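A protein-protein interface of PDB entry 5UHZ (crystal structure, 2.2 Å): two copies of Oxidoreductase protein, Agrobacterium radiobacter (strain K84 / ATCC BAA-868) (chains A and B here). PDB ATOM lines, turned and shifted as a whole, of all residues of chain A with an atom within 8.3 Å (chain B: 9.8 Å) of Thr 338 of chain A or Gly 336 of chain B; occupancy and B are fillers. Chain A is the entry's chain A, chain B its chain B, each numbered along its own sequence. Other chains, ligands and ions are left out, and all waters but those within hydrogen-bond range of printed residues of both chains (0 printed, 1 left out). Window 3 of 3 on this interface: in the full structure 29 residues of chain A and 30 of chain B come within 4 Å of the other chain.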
ATOM      1  N   ALA A 195     -16.238  12.231   0.121  1.00  0.00           N
ATOM      2  CA  ALA A 195     -17.185  12.845  -0.826  1.00  0.00           C
ATOM      3  C   ALA A 195     -18.461  12.023  -0.987  1.00  0.00           C
ATOM      4  O   ALA A 195     -19.561  12.573  -0.934  1.00  0.00           O
ATOM      5  CB  ALA A 195     -16.527  13.019  -2.184  1.00  0.00           C
ATOM      6  N   THR A 196     -18.303  10.712  -1.214  1.00  0.00           N
ATOM      7  CA  THR A 196     -19.443   9.792  -1.399  1.00  0.00           C
ATOM      8  C   THR A 196     -19.209   8.454  -0.704  1.00  0.00           C
ATOM      9  O   THR A 196     -18.073   8.034  -0.476  1.00  0.00           O
ATOM     10  CB  THR A 196     -19.766   9.524  -2.891  1.00  0.00           C
ATOM     11  OG1 THR A 196     -18.634   8.937  -3.537  1.00  0.00           O
ATOM     12  CG2 THR A 196     -20.153  10.811  -3.630  1.00  0.00           C
ATOM     13  N   LEU A 197     -20.314   7.783  -0.407  1.00  0.00           N
ATOM     14  CA  LEU A 197     -20.322   6.600   0.439  1.00  0.00           C
ATOM     15  C   LEU A 197     -21.459   5.668   0.022  1.00  0.00           C
ATOM     16  O   LEU A 197     -22.523   6.127  -0.392  1.00  0.00           O
ATOM     17  CB  LEU A 197     -20.488   7.057   1.889  1.00  0.00           C
ATOM     18  CG  LEU A 197     -20.671   6.048   3.030  1.00  0.00           C
ATOM     19  CD1 LEU A 197     -20.145   6.608   4.350  1.00  0.00           C
ATOM     20  CD2 LEU A 197     -22.122   5.612   3.207  1.00  0.00           C
ATOM     21  N   THR A 198     -21.226   4.362   0.133  1.00  0.00           N
ATOM     22  CA  THR A 198     -22.272   3.358  -0.070  1.00  0.00           C
ATOM     23  C   THR A 198     -22.077   2.194   0.917  1.00  0.00           C
ATOM     24  O   THR A 198     -20.950   1.747   1.138  1.00  0.00           O
ATOM     25  CB  THR A 198     -22.322   2.890  -1.544  1.00  0.00           C
ATOM     26  OG1 THR A 198     -23.414   1.987  -1.734  1.00  0.00           O
ATOM     27  CG2 THR A 198     -21.030   2.217  -1.967  1.00  0.00           C
ATOM     28  N   ALA A 199     -23.174   1.725   1.512  1.00  0.00           N
ATOM     29  CA  ALA A 199     -23.120   0.799   2.647  1.00  0.00           C
ATOM     30  C   ALA A 199     -24.145  -0.309   2.522  1.00  0.00           C
ATOM     31  O   ALA A 199     -25.213  -0.109   1.960  1.00  0.00           O
ATOM     32  CB  ALA A 199     -23.343   1.545   3.949  1.00  0.00           C
ATOM     33  N   ARG A 200     -23.792  -1.477   3.054  1.00  0.00           N
ATOM     34  CA  ARG A 200     -24.663  -2.649   3.099  1.00  0.00           C
ATOM     35  C   ARG A 200     -24.626  -3.189   4.516  1.00  0.00           C
ATOM     36  O   ARG A 200     -23.560  -3.237   5.120  1.00  0.00           O
ATOM     37  CB  ARG A 200     -24.161  -3.721   2.133  1.00  0.00           C
ATOM     38  CG  ARG A 200     -24.068  -3.273   0.679  1.00  0.00           C
ATOM     39  CD  ARG A 200     -25.438  -3.011   0.073  1.00  0.00           C
ATOM     40  NE  ARG A 200     -25.327  -2.737  -1.359  1.00  0.00           N
ATOM     41  CZ  ARG A 200     -24.951  -1.572  -1.890  1.00  0.00           C
ATOM     42  NH1 ARG A 200     -24.676  -0.515  -1.129  1.00  0.00           N
ATOM     43  NH2 ARG A 200     -24.867  -1.457  -3.213  1.00  0.00           N
ATOM     44  N   LEU A 217     -18.160   1.325   1.506  1.00  0.00           N
ATOM     45  CA  LEU A 217     -17.180   1.670   0.480  1.00  0.00           C
ATOM     46  C   LEU A 217     -17.126   3.197   0.386  1.00  0.00           C
ATOM     47  O   LEU A 217     -18.143   3.830   0.082  1.00  0.00           O
ATOM     48  CB  LEU A 217     -17.621   1.065  -0.850  1.00  0.00           C
ATOM     49  CG  LEU A 217     -16.871   1.411  -2.140  1.00  0.00           C
ATOM     50  CD1 LEU A 217     -15.462   0.849  -2.105  1.00  0.00           C
ATOM     51  CD2 LEU A 217     -17.624   0.876  -3.350  1.00  0.00           C
ATOM     52  N   ASP A 219     -15.464   6.883  -1.019  1.00  0.00           N
ATOM     53  CA  ASP A 219     -14.711   7.645  -2.015  1.00  0.00           C
ATOM     54  C   ASP A 219     -14.233   8.921  -1.343  1.00  0.00           C
ATOM     55  O   ASP A 219     -15.037   9.794  -1.026  1.00  0.00           O
ATOM     56  CB  ASP A 219     -15.587   7.981  -3.218  1.00  0.00           C
ATOM     57  CG  ASP A 219     -16.248   6.754  -3.807  1.00  0.00           C
ATOM     58  OD1 ASP A 219     -15.515   5.805  -4.148  1.00  0.00           O
ATOM     59  OD2 ASP A 219     -17.494   6.725  -3.930  1.00  0.00           O
ATOM     60  N   ALA A 328     -25.256   8.632   6.805  1.00  0.00           N
ATOM     61  CA  ALA A 328     -25.268   8.302   5.377  1.00  0.00           C
ATOM     62  C   ALA A 328     -25.228   6.798   5.118  1.00  0.00           C
ATOM     63  O   ALA A 328     -25.867   6.316   4.176  1.00  0.00           O
ATOM     64  CB  ALA A 328     -24.111   8.978   4.655  1.00  0.00           C
ATOM     65  N   GLU A 331     -28.690   5.385   5.712  1.00  0.00           N
ATOM     66  CA  GLU A 331     -29.475   5.797   4.546  1.00  0.00           C
ATOM     67  C   GLU A 331     -29.176   4.891   3.344  1.00  0.00           C
ATOM     68  O   GLU A 331     -30.091   4.316   2.763  1.00  0.00           O
ATOM     69  CB  GLU A 331     -29.185   7.267   4.202  1.00  0.00           C
ATOM     70  CG  GLU A 331     -30.153   7.925   3.232  1.00  0.00           C
ATOM     71  CD  GLU A 331     -29.743   9.352   2.883  1.00  0.00           C
ATOM     72  OE1 GLU A 331     -29.244  10.082   3.772  1.00  0.00           O
ATOM     73  OE2 GLU A 331     -29.920   9.743   1.709  1.00  0.00           O
ATOM     74  N   SER A 332     -27.891   4.748   3.014  1.00  0.00           N
ATOM     75  CA  SER A 332     -27.446   3.912   1.885  1.00  0.00           C
ATOM     76  C   SER A 332     -27.812   2.431   2.025  1.00  0.00           C
ATOM     77  O   SER A 332     -28.143   1.782   1.031  1.00  0.00           O
ATOM     78  CB  SER A 332     -25.936   4.027   1.700  1.00  0.00           C
ATOM     79  OG  SER A 332     -25.492   3.155   0.676  1.00  0.00           O
ATOM     80  N   ALA A 333     -27.737   1.904   3.249  1.00  0.00           N
ATOM     81  CA  ALA A 333     -28.066   0.504   3.516  1.00  0.00           C
ATOM     82  C   ALA A 333     -29.525   0.168   3.222  1.00  0.00           C
ATOM     83  O   ALA A 333     -29.820  -0.924   2.739  1.00  0.00           O
ATOM     84  CB  ALA A 333     -27.720   0.145   4.952  1.00  0.00           C
ATOM     85  N   ASN A 335     -31.489   2.062   1.057  1.00  0.00           N
ATOM     86  CA  ASN A 335     -31.736   2.417  -0.357  1.00  0.00           C
ATOM     87  C   ASN A 335     -31.028   1.504  -1.352  1.00  0.00           C
ATOM     88  O   ASN A 335     -31.537   1.284  -2.445  1.00  0.00           O
ATOM     89  CB  ASN A 335     -31.271   3.857  -0.652  1.00  0.00           C
ATOM     90  CG  ASN A 335     -32.007   4.908   0.166  1.00  0.00           C
ATOM     91  OD1 ASN A 335     -32.980   4.611   0.863  1.00  0.00           O
ATOM     92  ND2 ASN A 335     -31.539   6.153   0.081  1.00  0.00           N
ATOM     93  N   GLY A 336     -29.846   1.006  -0.987  1.00  0.00           N
ATOM     94  CA  GLY A 336     -28.924   0.371  -1.940  1.00  0.00           C
ATOM     95  C   GLY A 336     -28.184   1.376  -2.821  1.00  0.00           C
ATOM     96  O   GLY A 336     -27.523   0.987  -3.790  1.00  0.00           O
ATOM     97  N   ARG A 337     -28.257   2.661  -2.457  1.00  0.00           N
ATOM     98  CA  ARG A 337     -27.810   3.767  -3.304  1.00  0.00           C
ATOM     99  C   ARG A 337     -26.648   4.534  -2.652  1.00  0.00           C
ATOM    100  O   ARG A 337     -26.560   4.639  -1.420  1.00  0.00           O
ATOM    101  CB  ARG A 337     -28.982   4.717  -3.583  1.00  0.00           C
ATOM    102  N   THR A 338     -25.760   5.059  -3.495  1.00  0.00           N
ATOM    103  CA  THR A 338     -24.661   5.912  -3.054  1.00  0.00           C
ATOM    104  C   THR A 338     -25.210   7.239  -2.502  1.00  0.00           C
ATOM    105  O   THR A 338     -26.194   7.772  -3.019  1.00  0.00           O
ATOM    106  CB  THR A 338     -23.674   6.166  -4.218  1.00  0.00           C
ATOM    107  OG1 THR A 338     -23.154   4.910  -4.681  1.00  0.00           O
ATOM    108  CG2 THR A 338     -22.514   7.077  -3.798  1.00  0.00           C
ATOM    109  N   VAL A 339     -24.577   7.748  -1.444  1.00  0.00           N
ATOM    110  CA  VAL A 339     -25.031   8.953  -0.747  1.00  0.00           C
ATOM    111  C   VAL A 339     -23.948  10.036  -0.780  1.00  0.00           C
ATOM    112  O   VAL A 339     -22.805   9.810  -0.366  1.00  0.00           O
ATOM    113  CB  VAL A 339     -25.424   8.648   0.716  1.00  0.00           C
ATOM    114  CG1 VAL A 339     -25.778   9.926   1.475  1.00  0.00           C
ATOM    115  CG2 VAL A 339     -26.599   7.684   0.746  1.00  0.00           C
ATOM    116  N   ASP A 340     -24.337  11.212  -1.267  1.00  0.00           N
ATOM    117  CA  ASP A 340     -23.482  12.393  -1.295  1.00  0.00           C
ATOM    118  C   ASP A 340     -23.305  12.930   0.137  1.00  0.00           C
ATOM    119  O   ASP A 340     -24.285  13.289   0.800  1.00  0.00           O
ATOM    120  CB  ASP A 340     -24.126  13.455  -2.196  1.00  0.00           C
ATOM    121  CG  ASP A 340     -23.163  14.543  -2.611  1.00  0.00           C
ATOM    122  OD1 ASP A 340     -22.379  15.033  -1.768  1.00  0.00           O
ATOM    123  OD2 ASP A 340     -23.209  14.922  -3.798  1.00  0.00           O
ATOM    124  N   ILE A 341     -22.058  12.989   0.602  1.00  0.00           N
ATOM    125  CA  ILE A 341     -21.757  13.469   1.956  1.00  0.00           C
ATOM    126  C   ILE A 341     -21.765  15.002   1.996  1.00  0.00           C
ATOM    127  O   ILE A 341     -22.219  15.590   2.983  1.00  0.00           O
ATOM    128  CB  ILE A 341     -20.399  12.932   2.477  1.00  0.00           C
ATOM    129  CG1 ILE A 341     -20.343  11.391   2.415  1.00  0.00           C
ATOM    130  CG2 ILE A 341     -20.121  13.425   3.899  1.00  0.00           C
ATOM    131  CD1 ILE A 341     -21.442  10.672   3.176  1.00  0.00           C
ATOM    132  N   LEU B 197     -24.353  -4.702  -7.956  1.00  0.00           N
ATOM    133  CA  LEU B 197     -22.907  -4.509  -7.957  1.00  0.00           C
ATOM    134  C   LEU B 197     -22.554  -3.014  -8.028  1.00  0.00           C
ATOM    135  O   LEU B 197     -23.167  -2.276  -8.789  1.00  0.00           O
ATOM    136  CB  LEU B 197     -22.318  -5.270  -9.148  1.00  0.00           C
ATOM    137  CG  LEU B 197     -20.817  -5.153  -9.453  1.00  0.00           C
ATOM    138  CD1 LEU B 197     -20.326  -6.363 -10.242  1.00  0.00           C
ATOM    139  CD2 LEU B 197     -20.463  -3.864 -10.192  1.00  0.00           C
ATOM    140  N   THR B 198     -21.573  -2.575  -7.237  1.00  0.00           N
ATOM    141  CA  THR B 198     -21.052  -1.203  -7.310  1.00  0.00           C
ATOM    142  C   THR B 198     -19.516  -1.179  -7.228  1.00  0.00           C
ATOM    143  O   THR B 198     -18.927  -1.878  -6.400  1.00  0.00           O
ATOM    144  CB  THR B 198     -21.699  -0.284  -6.252  1.00  0.00           C
ATOM    145  OG1 THR B 198     -21.286   1.070  -6.474  1.00  0.00           O
ATOM    146  CG2 THR B 198     -21.350  -0.699  -4.844  1.00  0.00           C
ATOM    147  N   ALA B 199     -18.884  -0.365  -8.080  1.00  0.00           N
ATOM    148  CA  ALA B 199     -17.442  -0.450  -8.334  1.00  0.00           C
ATOM    149  C   ALA B 199     -16.756   0.904  -8.427  1.00  0.00           C
ATOM    150  O   ALA B 199     -17.366   1.901  -8.829  1.00  0.00           O
ATOM    151  CB  ALA B 199     -17.189  -1.230  -9.612  1.00  0.00           C
ATOM    152  N   ARG B 200     -15.478   0.925  -8.055  1.00  0.00           N
ATOM    153  CA  ARG B 200     -14.624   2.103  -8.196  1.00  0.00           C
ATOM    154  C   ARG B 200     -13.317   1.667  -8.841  1.00  0.00           C
ATOM    155  O   ARG B 200     -12.809   0.585  -8.532  1.00  0.00           O
ATOM    156  CB  ARG B 200     -14.347   2.724  -6.832  1.00  0.00           C
ATOM    157  CG  ARG B 200     -15.597   3.110  -6.050  1.00  0.00           C
ATOM    158  CD  ARG B 200     -16.359   4.263  -6.692  1.00  0.00           C
ATOM    159  NE  ARG B 200     -17.508   4.639  -5.870  1.00  0.00           N
ATOM    160  CZ  ARG B 200     -18.685   4.008  -5.843  1.00  0.00           C
ATOM    161  NH1 ARG B 200     -18.945   2.970  -6.638  1.00  0.00           N
ATOM    162  NH2 ARG B 200     -19.632   4.446  -5.021  1.00  0.00           N
ATOM    163  N   THR B 201     -12.788   2.487  -9.747  1.00  0.00           N
ATOM    164  CA  THR B 201     -11.522   2.193 -10.411  1.00  0.00           C
ATOM    165  C   THR B 201     -10.579   3.385 -10.414  1.00  0.00           C
ATOM    166  O   THR B 201     -10.993   4.531 -10.249  1.00  0.00           O
ATOM    167  CB  THR B 201     -11.723   1.711 -11.857  1.00  0.00           C
ATOM    168  OG1 THR B 201     -12.413   2.708 -12.622  1.00  0.00           O
ATOM    169  CG2 THR B 201     -12.516   0.418 -11.886  1.00  0.00           C
ATOM    170  N   THR B 215     -12.005  -1.717  -6.829  1.00  0.00           N
ATOM    171  CA  THR B 215     -12.665  -2.170  -5.612  1.00  0.00           C
ATOM    172  C   THR B 215     -14.155  -2.314  -5.945  1.00  0.00           C
ATOM    173  O   THR B 215     -14.796  -1.340  -6.354  1.00  0.00           O
ATOM    174  CB  THR B 215     -12.452  -1.161  -4.469  1.00  0.00           C
ATOM    175  OG1 THR B 215     -11.050  -0.907  -4.314  1.00  0.00           O
ATOM    176  CG2 THR B 215     -13.011  -1.678  -3.155  1.00  0.00           C
ATOM    177  N   LEU B 217     -18.064  -4.028  -4.805  1.00  0.00           N
ATOM    178  CA  LEU B 217     -18.919  -4.472  -3.697  1.00  0.00           C
ATOM    179  C   LEU B 217     -20.133  -5.209  -4.273  1.00  0.00           C
ATOM    180  O   LEU B 217     -20.938  -4.616  -4.995  1.00  0.00           O
ATOM    181  CB  LEU B 217     -19.352  -3.262  -2.878  1.00  0.00           C
ATOM    182  CG  LEU B 217     -20.342  -3.446  -1.727  1.00  0.00           C
ATOM    183  CD1 LEU B 217     -19.696  -4.183  -0.568  1.00  0.00           C
ATOM    184  CD2 LEU B 217     -20.860  -2.085  -1.277  1.00  0.00           C
ATOM    185  N   ALA B 328     -20.845  -4.551 -15.722  1.00  0.00           N
ATOM    186  CA  ALA B 328     -21.483  -3.769 -14.662  1.00  0.00           C
ATOM    187  C   ALA B 328     -20.460  -2.958 -13.871  1.00  0.00           C
ATOM    188  O   ALA B 328     -20.747  -1.833 -13.460  1.00  0.00           O
ATOM    189  CB  ALA B 328     -22.264  -4.673 -13.726  1.00  0.00           C
ATOM    190  N   ALA B 329     -19.273  -3.532 -13.667  1.00  0.00           N
ATOM    191  CA  ALA B 329     -18.204  -2.876 -12.910  1.00  0.00           C
ATOM    192  C   ALA B 329     -17.680  -1.640 -13.623  1.00  0.00           C
ATOM    193  O   ALA B 329     -17.562  -0.576 -13.010  1.00  0.00           O
ATOM    194  CB  ALA B 329     -17.063  -3.853 -12.644  1.00  0.00           C
ATOM    195  N   TYR B 330     -17.366  -1.786 -14.911  1.00  0.00           N
ATOM    196  CA  TYR B 330     -16.930  -0.648 -15.741  1.00  0.00           C
ATOM    197  C   TYR B 330     -17.971   0.454 -15.805  1.00  0.00           C
ATOM    198  O   TYR B 330     -17.618   1.631 -15.717  1.00  0.00           O
ATOM    199  CB  TYR B 330     -16.555  -1.090 -17.159  1.00  0.00           C
ATOM    200  CG  TYR B 330     -15.190  -1.723 -17.219  1.00  0.00           C
ATOM    201  CD1 TYR B 330     -14.050  -0.963 -16.974  1.00  0.00           C
ATOM    202  CD2 TYR B 330     -15.031  -3.081 -17.501  1.00  0.00           C
ATOM    203  CE1 TYR B 330     -12.788  -1.532 -17.011  1.00  0.00           C
ATOM    204  CE2 TYR B 330     -13.770  -3.661 -17.544  1.00  0.00           C
ATOM    205  CZ  TYR B 330     -12.652  -2.880 -17.299  1.00  0.00           C
ATOM    206  OH  TYR B 330     -11.400  -3.445 -17.334  1.00  0.00           O
ATOM    207  N   GLU B 331     -19.240   0.057 -15.941  1.00  0.00           N
ATOM    208  CA  GLU B 331     -20.383   0.988 -15.919  1.00  0.00           C
ATOM    209  C   GLU B 331     -20.474   1.724 -14.586  1.00  0.00           C
ATOM    210  O   GLU B 331     -20.497   2.942 -14.558  1.00  0.00           O
ATOM    211  CB  GLU B 331     -21.698   0.239 -16.195  1.00  0.00           C
ATOM    212  CG  GLU B 331     -22.909   1.125 -16.461  1.00  0.00           C
ATOM    213  CD  GLU B 331     -24.218   0.349 -16.506  1.00  0.00           C
ATOM    214  OE1 GLU B 331     -24.227  -0.804 -17.002  1.00  0.00           O
ATOM    215  OE2 GLU B 331     -25.247   0.899 -16.043  1.00  0.00           O
ATOM    216  N   SER B 332     -20.515   0.973 -13.486  1.00  0.00           N
ATOM    217  CA  SER B 332     -20.602   1.553 -12.139  1.00  0.00           C
ATOM    218  C   SER B 332     -19.436   2.486 -11.802  1.00  0.00           C
ATOM    219  O   SER B 332     -19.628   3.475 -11.098  1.00  0.00           O
ATOM    220  CB  SER B 332     -20.683   0.446 -11.084  1.00  0.00           C
ATOM    221  OG  SER B 332     -20.704   0.982  -9.773  1.00  0.00           O
ATOM    222  N   ALA B 333     -18.237   2.168 -12.291  1.00  0.00           N
ATOM    223  CA  ALA B 333     -17.040   2.981 -12.029  1.00  0.00           C
ATOM    224  C   ALA B 333     -17.103   4.345 -12.717  1.00  0.00           C
ATOM    225  O   ALA B 333     -16.709   5.353 -12.132  1.00  0.00           O
ATOM    226  CB  ALA B 333     -15.785   2.232 -12.451  1.00  0.00           C
ATOM    227  N   ALA B 334     -17.601   4.361 -13.950  1.00  0.00           N
ATOM    228  CA  ALA B 334     -17.829   5.601 -14.701  1.00  0.00           C
ATOM    229  C   ALA B 334     -18.996   6.422 -14.137  1.00  0.00           C
ATOM    230  O   ALA B 334     -18.898   7.645 -14.048  1.00  0.00           O
ATOM    231  CB  ALA B 334     -18.073   5.288 -16.174  1.00  0.00           C
ATOM    232  N   ASN B 335     -20.087   5.743 -13.769  1.00  0.00           N
ATOM    233  CA  ASN B 335     -21.306   6.390 -13.240  1.00  0.00           C
ATOM    234  C   ASN B 335     -21.157   6.836 -11.791  1.00  0.00           C
ATOM    235  O   ASN B 335     -21.526   7.953 -11.444  1.00  0.00           O
ATOM    236  CB  ASN B 335     -22.518   5.439 -13.310  1.00  0.00           C
ATOM    237  CG  ASN B 335     -22.947   5.108 -14.730  1.00  0.00           C
ATOM    238  OD1 ASN B 335     -22.323   5.528 -15.710  1.00  0.00           O
ATOM    239  ND2 ASN B 335     -24.025   4.335 -14.845  1.00  0.00           N
ATOM    240  N   GLY B 336     -20.635   5.944 -10.955  1.00  0.00           N
ATOM    241  CA  GLY B 336     -20.671   6.090  -9.497  1.00  0.00           C
ATOM    242  C   GLY B 336     -21.825   5.339  -8.837  1.00  0.00           C
ATOM    243  O   GLY B 336     -21.858   5.210  -7.605  1.00  0.00           O
ATOM    244  N   ARG B 337     -22.752   4.817  -9.650  1.00  0.00           N
ATOM    245  CA  ARG B 337     -24.014   4.245  -9.173  1.00  0.00           C
ATOM    246  C   ARG B 337     -24.000   2.705  -9.157  1.00  0.00           C
ATOM    247  O   ARG B 337     -23.215   2.059  -9.867  1.00  0.00           O
ATOM    248  CB  ARG B 337     -25.169   4.753 -10.044  1.00  0.00           C
ATOM    249  N   THR B 338     -24.874   2.138  -8.323  1.00  0.00           N
ATOM    250  CA  THR B 338     -25.078   0.694  -8.237  1.00  0.00           C
ATOM    251  C   THR B 338     -25.793   0.200  -9.497  1.00  0.00           C
ATOM    252  O   THR B 338     -26.655   0.891 -10.034  1.00  0.00           O
ATOM    253  CB  THR B 338     -25.904   0.325  -6.981  1.00  0.00           C
ATOM    254  OG1 THR B 338     -25.256   0.842  -5.809  1.00  0.00           O
ATOM    255  CG2 THR B 338     -26.058  -1.187  -6.837  1.00  0.00           C
ATOM    256  N   VAL B 339     -25.421  -0.992  -9.958  1.00  0.00           N
ATOM    257  CA  VAL B 339     -25.920  -1.562 -11.211  1.00  0.00           C
ATOM    258  C   VAL B 339     -26.639  -2.884 -10.947  1.00  0.00           C
ATOM    259  O   VAL B 339     -26.079  -3.786 -10.324  1.00  0.00           O
ATOM    260  CB  VAL B 339     -24.761  -1.771 -12.209  1.00  0.00           C
ATOM    261  CG1 VAL B 339     -25.208  -2.552 -13.444  1.00  0.00           C
ATOM    262  CG2 VAL B 339     -24.182  -0.418 -12.611  1.00  0.00           C
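O of Asp 219 of chain A lies within hydrogen-bond range of N of Ala 195 of chain A. The side-chain hydroxyl (OG) of Ser 332 of chain B lies close to the side-chain hydroxyl (OG1) of Thr 198 of chain B. O of Gly 336 of chain B lies within hydrogen-bond range of NH2 of Arg 200 of chain B, 3.5 Å away. OG1 of Thr 198 of chain B sits at hydrogen-bond distance from NH1 of Arg 200 of chain B, 3.0 Å away. The backbone carbonyl oxygen (O) of Thr 215 of chain B lies within hydrogen-bond range of the backbone NH (N) of Arg 200 of chain B. N of Leu 217 of chain A lies within hydrogen-bond range of O of Thr 198 of chain A, 2.8 Å away.
Printed residues of chain B that touch a printed residue of chain A: Thr 198, Arg 200, Thr 215, Leu 217, Gly 336 and Thr 338. Of the 19 printed residues of chain A, 5 touch a printed residue of chain B. Printed residues of chain A that touch a printed residue of chain B: Arg 200, Leu 217, Asp 219, Gly 336 and Thr 338.
Of chain A, only Thr 338 (3.2 Å) comes within 4 Å of Gly 336 of chain B. No residue of chain B comes within 4 Å of Arg 337 of chain A. No residue of chain B comes within 4 Å of Val 339 of chain A. No residue of chain A comes within 4 Å of Arg 337 of chain B. Of the printed residues of chain A, Leu 217 of chain B touches Arg 200 (3.9 Å). Of the printed residues of chain A, Thr 338 of chain B touches Arg 200 and Gly 336.
Arg 200 of chain A touches Thr 198 of chain B, but with the chains exchanged Thr 198 of chain A does not touch Arg 200 of chain B (4.03 Å). Arg 200 of chain A touches Leu 217 of chain B, but with the chains exchanged Leu 217 of chain A does not touch Arg 200 of chain B (4.05 Å). Arg 200 of chain A touches Thr 338 of chain B, and with the chains exchanged Thr 338 of chain A touches Arg 200 of chain B. Gly 336 of chain A touches Thr 338 of chain B, and with the chains exchanged Thr 338 of chain A touches Gly 336 of chain B. Of the 8 pairs that touch across the chains among the printed residues, 4 have their exchanged pair printed and touching as well.
OG1 of Thr 338 of chain B lies within hydrogen-bond range of NH2 of Arg 200 of chain A, 3.5 Å away. O of Gly 336 of chain B is in hydrogen-bond range of OG1 of Thr 338 of chain A (3.2 Å). OD2 of Asp 219 of chain A lies within salt-bridge range of NE of Arg 200 of chain B. O of Gly 336 of chain A is in hydrogen-bond range of OG1 of Thr 338 of chain B.
Among the printed residues, merely in contact across the chains: Arg 200 of chain A with Thr 198 of chain B (3.95 Å), Arg 200 of chain A with Leu 217 of chain B (3.9 Å), Leu 217 of chain A with Thr 215 of chain B (3.7 Å) and Thr 338 of chain A with Arg 200 of chain B (3.6 Å).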
